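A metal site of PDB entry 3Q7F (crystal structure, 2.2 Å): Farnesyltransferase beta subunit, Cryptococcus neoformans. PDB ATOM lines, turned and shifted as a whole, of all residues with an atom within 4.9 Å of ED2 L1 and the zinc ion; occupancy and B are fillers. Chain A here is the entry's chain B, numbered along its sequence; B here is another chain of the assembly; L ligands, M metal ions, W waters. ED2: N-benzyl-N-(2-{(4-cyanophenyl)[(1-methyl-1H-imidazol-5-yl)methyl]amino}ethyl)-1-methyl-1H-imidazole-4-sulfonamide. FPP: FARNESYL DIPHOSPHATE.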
ATOM      1  N   PHE A  81       7.906  11.249  -9.200  1.00  0.00           N
ATOM      2  CA  PHE A  81       7.059  11.816  -8.164  1.00  0.00           C
ATOM      3  C   PHE A  81       6.674  13.278  -8.420  1.00  0.00           C
ATOM      4  O   PHE A  81       6.000  13.913  -7.599  1.00  0.00           O
ATOM      5  CB  PHE A  81       7.708  11.669  -6.785  1.00  0.00           C
ATOM      6  CG  PHE A  81       7.399  10.366  -6.105  1.00  0.00           C
ATOM      7  CD1 PHE A  81       6.388  10.292  -5.147  1.00  0.00           C
ATOM      8  CD2 PHE A  81       8.111   9.213  -6.434  1.00  0.00           C
ATOM      9  CE1 PHE A  81       6.103   9.085  -4.503  1.00  0.00           C
ATOM     10  CE2 PHE A  81       7.823   7.994  -5.795  1.00  0.00           C
ATOM     11  CZ  PHE A  81       6.815   7.932  -4.833  1.00  0.00           C
ATOM     12  N   LEU A  84       3.287  14.601  -7.976  1.00  0.00           N
ATOM     13  CA  LEU A  84       2.876  14.969  -6.615  1.00  0.00           C
ATOM     14  C   LEU A  84       3.624  16.190  -6.070  1.00  0.00           C
ATOM     15  O   LEU A  84       3.627  16.429  -4.857  1.00  0.00           O
ATOM     16  CB  LEU A  84       3.030  13.773  -5.659  1.00  0.00           C
ATOM     17  CG  LEU A  84       2.081  12.573  -5.841  1.00  0.00           C
ATOM     18  CD1 LEU A  84       2.454  11.449  -4.877  1.00  0.00           C
ATOM     19  CD2 LEU A  84       0.621  12.971  -5.660  1.00  0.00           C
ATOM     20  N   SER A  87       1.726  18.374  -3.953  1.00  0.00           N
ATOM     21  CA  SER A  87       1.170  17.648  -2.810  1.00  0.00           C
ATOM     22  C   SER A  87       2.211  17.172  -1.787  1.00  0.00           C
ATOM     23  O   SER A  87       1.962  16.217  -1.051  1.00  0.00           O
ATOM     24  CB  SER A  87       0.363  16.444  -3.302  1.00  0.00           C
ATOM     25  OG  SER A  87      -0.800  16.863  -3.999  1.00  0.00           O
ATOM     26  N   TRP A  90       1.297  16.428   1.859  1.00  0.00           N
ATOM     27  CA  TRP A  90       0.620  15.136   2.002  1.00  0.00           C
ATOM     28  C   TRP A  90       1.624  13.996   2.128  1.00  0.00           C
ATOM     29  O   TRP A  90       1.423  13.083   2.923  1.00  0.00           O
ATOM     30  CB  TRP A  90      -0.345  14.871   0.848  1.00  0.00           C
ATOM     31  CG  TRP A  90      -1.619  15.630   0.972  1.00  0.00           C
ATOM     32  CD1 TRP A  90      -1.981  16.725   0.240  1.00  0.00           C
ATOM     33  CD2 TRP A  90      -2.689  15.366   1.872  1.00  0.00           C
ATOM     34  NE1 TRP A  90      -3.224  17.155   0.636  1.00  0.00           N
ATOM     35  CE2 TRP A  90      -3.679  16.343   1.637  1.00  0.00           C
ATOM     36  CE3 TRP A  90      -2.921  14.396   2.860  1.00  0.00           C
ATOM     37  CZ2 TRP A  90      -4.888  16.384   2.354  1.00  0.00           C
ATOM     38  CZ3 TRP A  90      -4.117  14.440   3.581  1.00  0.00           C
ATOM     39  CH2 TRP A  90      -5.086  15.430   3.318  1.00  0.00           C
ATOM     40  N   LEU A  91       2.722  14.069   1.364  1.00  0.00           N
ATOM     41  CA  LEU A  91       3.795  13.074   1.476  1.00  0.00           C
ATOM     42  C   LEU A  91       4.400  13.098   2.890  1.00  0.00           C
ATOM     43  O   LEU A  91       4.711  12.048   3.454  1.00  0.00           O
ATOM     44  CB  LEU A  91       4.868  13.298   0.405  1.00  0.00           C
ATOM     45  CG  LEU A  91       4.507  12.892  -1.026  1.00  0.00           C
ATOM     46  CD1 LEU A  91       5.326  13.664  -2.050  1.00  0.00           C
ATOM     47  CD2 LEU A  91       4.666  11.392  -1.228  1.00  0.00           C
ATOM     48  N   TRP A  94       1.432  11.577   5.233  1.00  0.00           N
ATOM     49  CA  TRP A  94       1.319  10.125   5.094  1.00  0.00           C
ATOM     50  C   TRP A  94       2.442   9.390   5.815  1.00  0.00           C
ATOM     51  O   TRP A  94       2.202   8.366   6.447  1.00  0.00           O
ATOM     52  CB  TRP A  94       1.236   9.685   3.619  1.00  0.00           C
ATOM     53  CG  TRP A  94       0.047  10.260   2.868  1.00  0.00           C
ATOM     54  CD1 TRP A  94      -1.207  10.485   3.365  1.00  0.00           C
ATOM     55  CD2 TRP A  94       0.016  10.668   1.487  1.00  0.00           C
ATOM     56  NE1 TRP A  94      -2.009  11.009   2.392  1.00  0.00           N
ATOM     57  CE2 TRP A  94      -1.288  11.128   1.233  1.00  0.00           C
ATOM     58  CE3 TRP A  94       0.961  10.687   0.462  1.00  0.00           C
ATOM     59  CZ2 TRP A  94      -1.677  11.614  -0.027  1.00  0.00           C
ATOM     60  CZ3 TRP A  94       0.579  11.168  -0.792  1.00  0.00           C
ATOM     61  CH2 TRP A  94      -0.733  11.628  -1.023  1.00  0.00           C
ATOM     62  N   ARG A 197     -14.163  18.402   0.426  1.00  0.00           N
ATOM     63  CA  ARG A 197     -12.807  18.144   0.954  1.00  0.00           C
ATOM     64  C   ARG A 197     -12.189  19.427   1.510  1.00  0.00           C
ATOM     65  O   ARG A 197     -11.485  19.393   2.527  1.00  0.00           O
ATOM     66  CB  ARG A 197     -11.875  17.594  -0.122  1.00  0.00           C
ATOM     67  CG  ARG A 197     -12.202  16.205  -0.632  1.00  0.00           C
ATOM     68  CD  ARG A 197     -11.264  15.833  -1.777  1.00  0.00           C
ATOM     69  NE  ARG A 197     -11.143  16.920  -2.747  1.00  0.00           N
ATOM     70  CZ  ARG A 197     -10.145  17.082  -3.601  1.00  0.00           C
ATOM     71  NH1 ARG A 197      -9.132  16.220  -3.635  1.00  0.00           N
ATOM     72  NH2 ARG A 197     -10.143  18.130  -4.421  1.00  0.00           N
ATOM     73  N   ASP A 323     -11.009  -1.289  -2.034  1.00  0.00           N
ATOM     74  CA  ASP A 323      -9.743  -0.571  -2.055  1.00  0.00           C
ATOM     75  C   ASP A 323      -9.333  -0.296  -0.606  1.00  0.00           C
ATOM     76  O   ASP A 323     -10.126   0.217   0.186  1.00  0.00           O
ATOM     77  CB  ASP A 323      -9.906   0.728  -2.839  1.00  0.00           C
ATOM     78  CG  ASP A 323      -8.620   1.532  -2.944  1.00  0.00           C
ATOM     79  OD1 ASP A 323      -7.721   1.415  -2.080  1.00  0.00           O
ATOM     80  OD2 ASP A 323      -8.528   2.316  -3.908  1.00  0.00           O
ATOM     81  N   CYS A 325      -7.624   1.935   0.846  1.00  0.00           N
ATOM     82  CA  CYS A 325      -7.673   3.293   1.388  1.00  0.00           C
ATOM     83  C   CYS A 325      -9.035   3.653   1.973  1.00  0.00           C
ATOM     84  O   CYS A 325      -9.128   4.505   2.863  1.00  0.00           O
ATOM     85  CB  CYS A 325      -7.200   4.360   0.374  1.00  0.00           C
ATOM     86  SG  CYS A 325      -8.264   4.617  -1.073  1.00  0.00           S
ATOM     87  N   TYR A 326     -10.086   2.968   1.515  1.00  0.00           N
ATOM     88  CA  TYR A 326     -11.440   3.212   2.030  1.00  0.00           C
ATOM     89  C   TYR A 326     -11.634   2.663   3.439  1.00  0.00           C
ATOM     90  O   TYR A 326     -12.644   2.932   4.087  1.00  0.00           O
ATOM     91  CB  TYR A 326     -12.515   2.707   1.066  1.00  0.00           C
ATOM     92  CG  TYR A 326     -12.483   3.428  -0.270  1.00  0.00           C
ATOM     93  CD1 TYR A 326     -12.618   4.808  -0.343  1.00  0.00           C
ATOM     94  CD2 TYR A 326     -12.276   2.721  -1.464  1.00  0.00           C
ATOM     95  CE1 TYR A 326     -12.570   5.475  -1.562  1.00  0.00           C
ATOM     96  CE2 TYR A 326     -12.231   3.374  -2.688  1.00  0.00           C
ATOM     97  CZ  TYR A 326     -12.369   4.750  -2.731  1.00  0.00           C
ATOM     98  OH  TYR A 326     -12.325   5.411  -3.934  1.00  0.00           O
ATOM     99  N   TRP A 329     -11.448   6.073   4.798  1.00  0.00           N
ATOM    100  CA  TRP A 329     -12.515   6.975   4.338  1.00  0.00           C
ATOM    101  C   TRP A 329     -13.921   6.515   4.701  1.00  0.00           C
ATOM    102  O   TRP A 329     -14.734   7.303   5.173  1.00  0.00           O
ATOM    103  CB  TRP A 329     -12.423   7.296   2.841  1.00  0.00           C
ATOM    104  CG  TRP A 329     -11.088   7.841   2.419  1.00  0.00           C
ATOM    105  CD1 TRP A 329     -10.216   7.275   1.530  1.00  0.00           C
ATOM    106  CD2 TRP A 329     -10.466   9.058   2.866  1.00  0.00           C
ATOM    107  NE1 TRP A 329      -9.095   8.061   1.386  1.00  0.00           N
ATOM    108  CE2 TRP A 329      -9.228   9.159   2.187  1.00  0.00           C
ATOM    109  CE3 TRP A 329     -10.846  10.068   3.752  1.00  0.00           C
ATOM    110  CZ2 TRP A 329      -8.347  10.233   2.395  1.00  0.00           C
ATOM    111  CZ3 TRP A 329      -9.965  11.142   3.960  1.00  0.00           C
ATOM    112  CH2 TRP A 329      -8.745  11.217   3.280  1.00  0.00           C
ATOM    113  N   ASP A 400      -3.632  -0.446  -2.485  1.00  0.00           N
ATOM    114  CA  ASP A 400      -5.036  -0.464  -2.876  1.00  0.00           C
ATOM    115  C   ASP A 400      -5.599  -1.895  -2.813  1.00  0.00           C
ATOM    116  O   ASP A 400      -6.548  -2.167  -2.066  1.00  0.00           O
ATOM    117  CB  ASP A 400      -5.126   0.156  -4.287  1.00  0.00           C
ATOM    118  CG  ASP A 400      -6.456  -0.095  -5.016  1.00  0.00           C
ATOM    119  OD1 ASP A 400      -7.342  -0.842  -4.531  1.00  0.00           O
ATOM    120  OD2 ASP A 400      -6.607   0.477  -6.107  1.00  0.00           O
ATOM    121  N   ASP A 407       1.986   2.417  -2.024  1.00  0.00           N
ATOM    122  CA  ASP A 407       2.423   3.817  -1.986  1.00  0.00           C
ATOM    123  C   ASP A 407       2.217   4.420  -0.601  1.00  0.00           C
ATOM    124  O   ASP A 407       1.616   3.793   0.280  1.00  0.00           O
ATOM    125  CB  ASP A 407       1.705   4.641  -3.085  1.00  0.00           C
ATOM    126  CG  ASP A 407       0.195   4.593  -2.960  1.00  0.00           C
ATOM    127  OD1 ASP A 407      -0.338   5.031  -1.929  1.00  0.00           O
ATOM    128  OD2 ASP A 407      -0.472   4.115  -3.912  1.00  0.00           O
ATOM    129  N   GLN A 408       2.713   5.646  -0.413  1.00  0.00           N
ATOM    130  CA  GLN A 408       2.615   6.342   0.869  1.00  0.00           C
ATOM    131  C   GLN A 408       1.171   6.628   1.268  1.00  0.00           C
ATOM    132  O   GLN A 408       0.795   6.467   2.435  1.00  0.00           O
ATOM    133  CB  GLN A 408       3.411   7.661   0.831  1.00  0.00           C
ATOM    134  CG  GLN A 408       4.924   7.490   0.661  1.00  0.00           C
ATOM    135  CD  GLN A 408       5.364   7.425  -0.801  1.00  0.00           C
ATOM    136  OE1 GLN A 408       4.558   7.191  -1.699  1.00  0.00           O
ATOM    137  NE2 GLN A 408       6.650   7.640  -1.030  1.00  0.00           N
ATOM    138  N   TYR A 409       0.363   7.040   0.285  1.00  0.00           N
ATOM    139  CA  TYR A 409      -1.045   7.338   0.502  1.00  0.00           C
ATOM    140  C   TYR A 409      -1.814   6.112   0.996  1.00  0.00           C
ATOM    141  O   TYR A 409      -2.596   6.209   1.943  1.00  0.00           O
ATOM    142  CB  TYR A 409      -1.671   7.894  -0.792  1.00  0.00           C
ATOM    143  CG  TYR A 409      -3.186   7.913  -0.802  1.00  0.00           C
ATOM    144  CD1 TYR A 409      -3.885   9.029  -0.355  1.00  0.00           C
ATOM    145  CD2 TYR A 409      -3.913   6.823  -1.277  1.00  0.00           C
ATOM    146  CE1 TYR A 409      -5.279   9.056  -0.368  1.00  0.00           C
ATOM    147  CE2 TYR A 409      -5.305   6.833  -1.289  1.00  0.00           C
ATOM    148  CZ  TYR A 409      -5.977   7.954  -0.833  1.00  0.00           C
ATOM    149  OH  TYR A 409      -7.352   7.979  -0.835  1.00  0.00           O
ATOM    150  N   HIS A 410      -1.571   4.967   0.366  1.00  0.00           N
ATOM    151  CA  HIS A 410      -2.243   3.734   0.778  1.00  0.00           C
ATOM    152  C   HIS A 410      -1.681   3.155   2.071  1.00  0.00           C
ATOM    153  O   HIS A 410      -2.410   2.534   2.832  1.00  0.00           O
ATOM    154  CB  HIS A 410      -2.255   2.713  -0.357  1.00  0.00           C
ATOM    155  CG  HIS A 410      -3.288   3.002  -1.393  1.00  0.00           C
ATOM    156  ND1 HIS A 410      -2.989   3.556  -2.620  1.00  0.00           N
ATOM    157  CD2 HIS A 410      -4.635   2.845  -1.375  1.00  0.00           C
ATOM    158  CE1 HIS A 410      -4.099   3.721  -3.310  1.00  0.00           C
ATOM    159  NE2 HIS A 410      -5.121   3.301  -2.577  1.00  0.00           N
ATOM    160  N   TYR B 123      -8.086  16.900 -11.419  1.00  0.00           N
ATOM    161  CA  TYR B 123      -9.077  17.881 -10.952  1.00  0.00           C
ATOM    162  C   TYR B 123      -8.942  19.183 -11.743  1.00  0.00           C
ATOM    163  O   TYR B 123      -9.943  19.815 -12.095  1.00  0.00           O
ATOM    164  CB  TYR B 123      -8.846  18.228  -9.483  1.00  0.00           C
ATOM    165  CG  TYR B 123      -9.331  17.218  -8.464  1.00  0.00           C
ATOM    166  CD1 TYR B 123     -10.607  17.318  -7.921  1.00  0.00           C
ATOM    167  CD2 TYR B 123      -8.496  16.182  -8.025  1.00  0.00           C
ATOM    168  CE1 TYR B 123     -11.063  16.403  -6.975  1.00  0.00           C
ATOM    169  CE2 TYR B 123      -8.942  15.256  -7.080  1.00  0.00           C
ATOM    170  CZ  TYR B 123     -10.220  15.367  -6.560  1.00  0.00           C
ATOM    171  OH  TYR B 123     -10.675  14.462  -5.622  1.00  0.00           O
HETATM  172  CAB ED2 L   1      -5.761   4.963  -8.044  1.00  0.00           C
HETATM  173  NBH ED2 L   1      -6.033   5.344  -6.653  1.00  0.00           N
HETATM  174  CAQ ED2 L   1      -6.547   4.508  -5.689  1.00  0.00           C
HETATM  175  NAX ED2 L   1      -6.726   5.202  -4.593  1.00  0.00           N
HETATM  176  CAP ED2 L   1      -6.038   6.408  -4.744  1.00  0.00           C
HETATM  177  CBC ED2 L   1      -5.670   6.524  -6.044  1.00  0.00           C
HETATM  178  CAW ED2 L   1      -4.970   7.676  -6.677  1.00  0.00           C
HETATM  179  NBE ED2 L   1      -4.463   8.657  -5.707  1.00  0.00           N
HETATM  180  CBB ED2 L   1      -3.170   8.554  -5.167  1.00  0.00           C
HETATM  181  CAN ED2 L   1      -2.580   9.655  -4.536  1.00  0.00           C
HETATM  182  CAL ED2 L   1      -1.225   9.545  -3.907  1.00  0.00           C
HETATM  183  CAZ ED2 L   1      -0.549   8.384  -3.990  1.00  0.00           C
HETATM  184  CAF ED2 L   1       0.820   8.258  -3.369  1.00  0.00           C
HETATM  185  NAC ED2 L   1       1.868   8.152  -2.890  1.00  0.00           N
HETATM  186  CAM ED2 L   1      -1.161   7.218  -4.675  1.00  0.00           C
HETATM  187  CAO ED2 L   1      -2.452   7.325  -5.245  1.00  0.00           C
HETATM  188  CAT ED2 L   1      -5.254   9.926  -5.547  1.00  0.00           C
HETATM  189  CAU ED2 L   1      -5.632  10.120  -4.073  1.00  0.00           C
HETATM  190  NBF ED2 L   1      -6.279  11.442  -3.831  1.00  0.00           N
HETATM  191  SBI ED2 L   1      -7.933  11.381  -3.900  1.00  0.00           S
HETATM  192  OAD ED2 L   1      -8.393  11.784  -2.591  1.00  0.00           O
HETATM  193  OAE ED2 L   1      -8.457  12.303  -4.887  1.00  0.00           O
HETATM  194  CBD ED2 L   1      -8.485   9.735  -4.181  1.00  0.00           C
HETATM  195  CAS ED2 L   1      -8.604   9.075  -5.446  1.00  0.00           C
HETATM  196  NBG ED2 L   1      -9.019   7.747  -5.163  1.00  0.00           N
HETATM  197  CAA ED2 L   1      -9.257   6.700  -6.128  1.00  0.00           C
HETATM  198  CAR ED2 L   1      -9.144   7.619  -3.765  1.00  0.00           C
HETATM  199  NAY ED2 L   1      -8.798   8.815  -3.205  1.00  0.00           N
HETATM  200  CAV ED2 L   1      -5.722  12.568  -4.607  1.00  0.00           C
HETATM  201  CBA ED2 L   1      -4.787  13.338  -3.715  1.00  0.00           C
HETATM  202  CAJ ED2 L   1      -5.177  13.704  -2.437  1.00  0.00           C
HETATM  203  CAH ED2 L   1      -4.312  14.404  -1.632  1.00  0.00           C
HETATM  204  CAG ED2 L   1      -3.035  14.731  -2.102  1.00  0.00           C
HETATM  205  CAI ED2 L   1      -2.637  14.350  -3.351  1.00  0.00           C
HETATM  206  CAK ED2 L   1      -3.516  13.658  -4.182  1.00  0.00           C
HETATM  207  C1  FPP L   2     -12.333   8.455  -7.285  1.00  0.00           C
HETATM  208  O1  FPP L   2     -11.457   7.884  -8.182  1.00  0.00           O
HETATM  209  C2  FPP L   2     -11.788   9.776  -6.848  1.00  0.00           C
HETATM  210  C3  FPP L   2     -12.508  10.636  -6.061  1.00  0.00           C
HETATM  211  C4  FPP L   2     -13.649  11.362  -6.677  1.00  0.00           C
HETATM  212  C5  FPP L   2     -11.817  11.306  -4.923  1.00  0.00           C
HETATM  213  C6  FPP L   2     -12.199  10.665  -3.627  1.00  0.00           C
HETATM  214  C7  FPP L   2     -12.023  11.659  -2.514  1.00  0.00           C
HETATM  215  C8  FPP L   2     -11.226  11.424  -1.416  1.00  0.00           C
HETATM  216  C10 FPP L   2     -10.738  10.047  -1.109  1.00  0.00           C
HETATM  217  C9  FPP L   2     -11.317  12.415  -0.294  1.00  0.00           C
HETATM  218  C11 FPP L   2      -9.969  12.800   0.215  1.00  0.00           C
HETATM  219  C12 FPP L   2     -10.123  13.847   1.264  1.00  0.00           C
HETATM  220  C13 FPP L   2      -9.113  14.721   1.582  1.00  0.00           C
HETATM  221  C14 FPP L   2      -9.123  15.387   2.916  1.00  0.00           C
HETATM  222  C15 FPP L   2      -8.081  15.094   0.577  1.00  0.00           C
HETATM  223  PA  FPP L   2     -11.566   6.394  -8.630  1.00  0.00           P
HETATM  224  O1A FPP L   2     -12.678   6.275  -9.696  1.00  0.00           O
HETATM  225  O2A FPP L   2     -10.217   5.988  -9.266  1.00  0.00           O
HETATM  226  O3A FPP L   2     -11.826   5.501  -7.377  1.00  0.00           O
HETATM  227  PB  FPP L   2     -13.050   4.543  -7.189  1.00  0.00           P
HETATM  228  O1B FPP L   2     -13.139   3.578  -8.350  1.00  0.00           O
HETATM  229  O2B FPP L   2     -12.826   3.760  -5.925  1.00  0.00           O
HETATM  230  O3B FPP L   2     -14.328   5.341  -7.097  1.00  0.00           O
HETATM  231 ZN    ZN M   1      -7.090   3.765  -2.883  1.00  0.00          ZN
HETATM  232  O   HOH W   1      -9.057   3.838  -8.043  1.00  0.00           O
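The zinc ion is bound by NE2 of His 410 (2.0 Å), NAX of ED2 L1 (2.3 Å), OD2 of Asp 323 (2.3 Å), SG of Cys 325 (2.3 Å) and OD1 of Asp 323 (2.6 Å).
The zinc ion has five donor atoms within binding distance.
OH of Tyr 409 lies within hydrogen-bond range of NAY of ED2 L1, at 2.9 Å.
OE1 of Gln 408 lies close to NAC of ED2 L1.
The side-chain hydroxyl of Tyr 123 of chain B sits at hydrogen-bond distance from an oxygen (OAE) of ED2 L1 (3.2 Å).
The side-chain hydroxyl (OH) of Tyr 326 sits at hydrogen-bond distance from an oxygen (O2B) of FPP L2.
Residues that only touch ED2 L1: Ser 87 (3.2 Å), Trp 90 (3.3 Å), Asp 407 (3.3 Å), Trp 94 (3.6 Å), Tyr 326 (3.9 Å) and Leu 84 (3.9 Å).
Hydrophobic or aromatic side chains within 4 Å of ED2 L1: Leu 84, Trp 90, Trp 94, Tyr 409, His 410 and Tyr 123 of chain B.
Along chain A the residues within 4 Å of ED2 L1 span positions 84 to 410.
Residues that only touch the zinc ion: Tyr 409.
Of the 17 residues printed, 4 come within 4 Å of the zinc ion.
The nearest printed residue that does not touch the zinc ion is Asp 400 (4.3 Å).
The side-chain carboxylate (OD1) of Asp 407 sits at hydrogen-bond distance from the backbone NH (N) of Tyr 409.
N of His 410 sits at hydrogen-bond distance from OD1 of Asp 407, at 2.6 Å.
The side-chain hydroxyl (OH) of Tyr 123 of chain B lies within hydrogen-bond range of the guanidinium group (NH1) of Arg 197 (3.1 Å).
The side-chain sulfur of Cys 325 sits close to the side-chain hydroxyl of Tyr 409 (3.5 Å).
The indole nitrogen (NE1) of Trp 329 lies within hydrogen-bond range of the side-chain hydroxyl (OH) of Tyr 409, at 2.8 Å.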
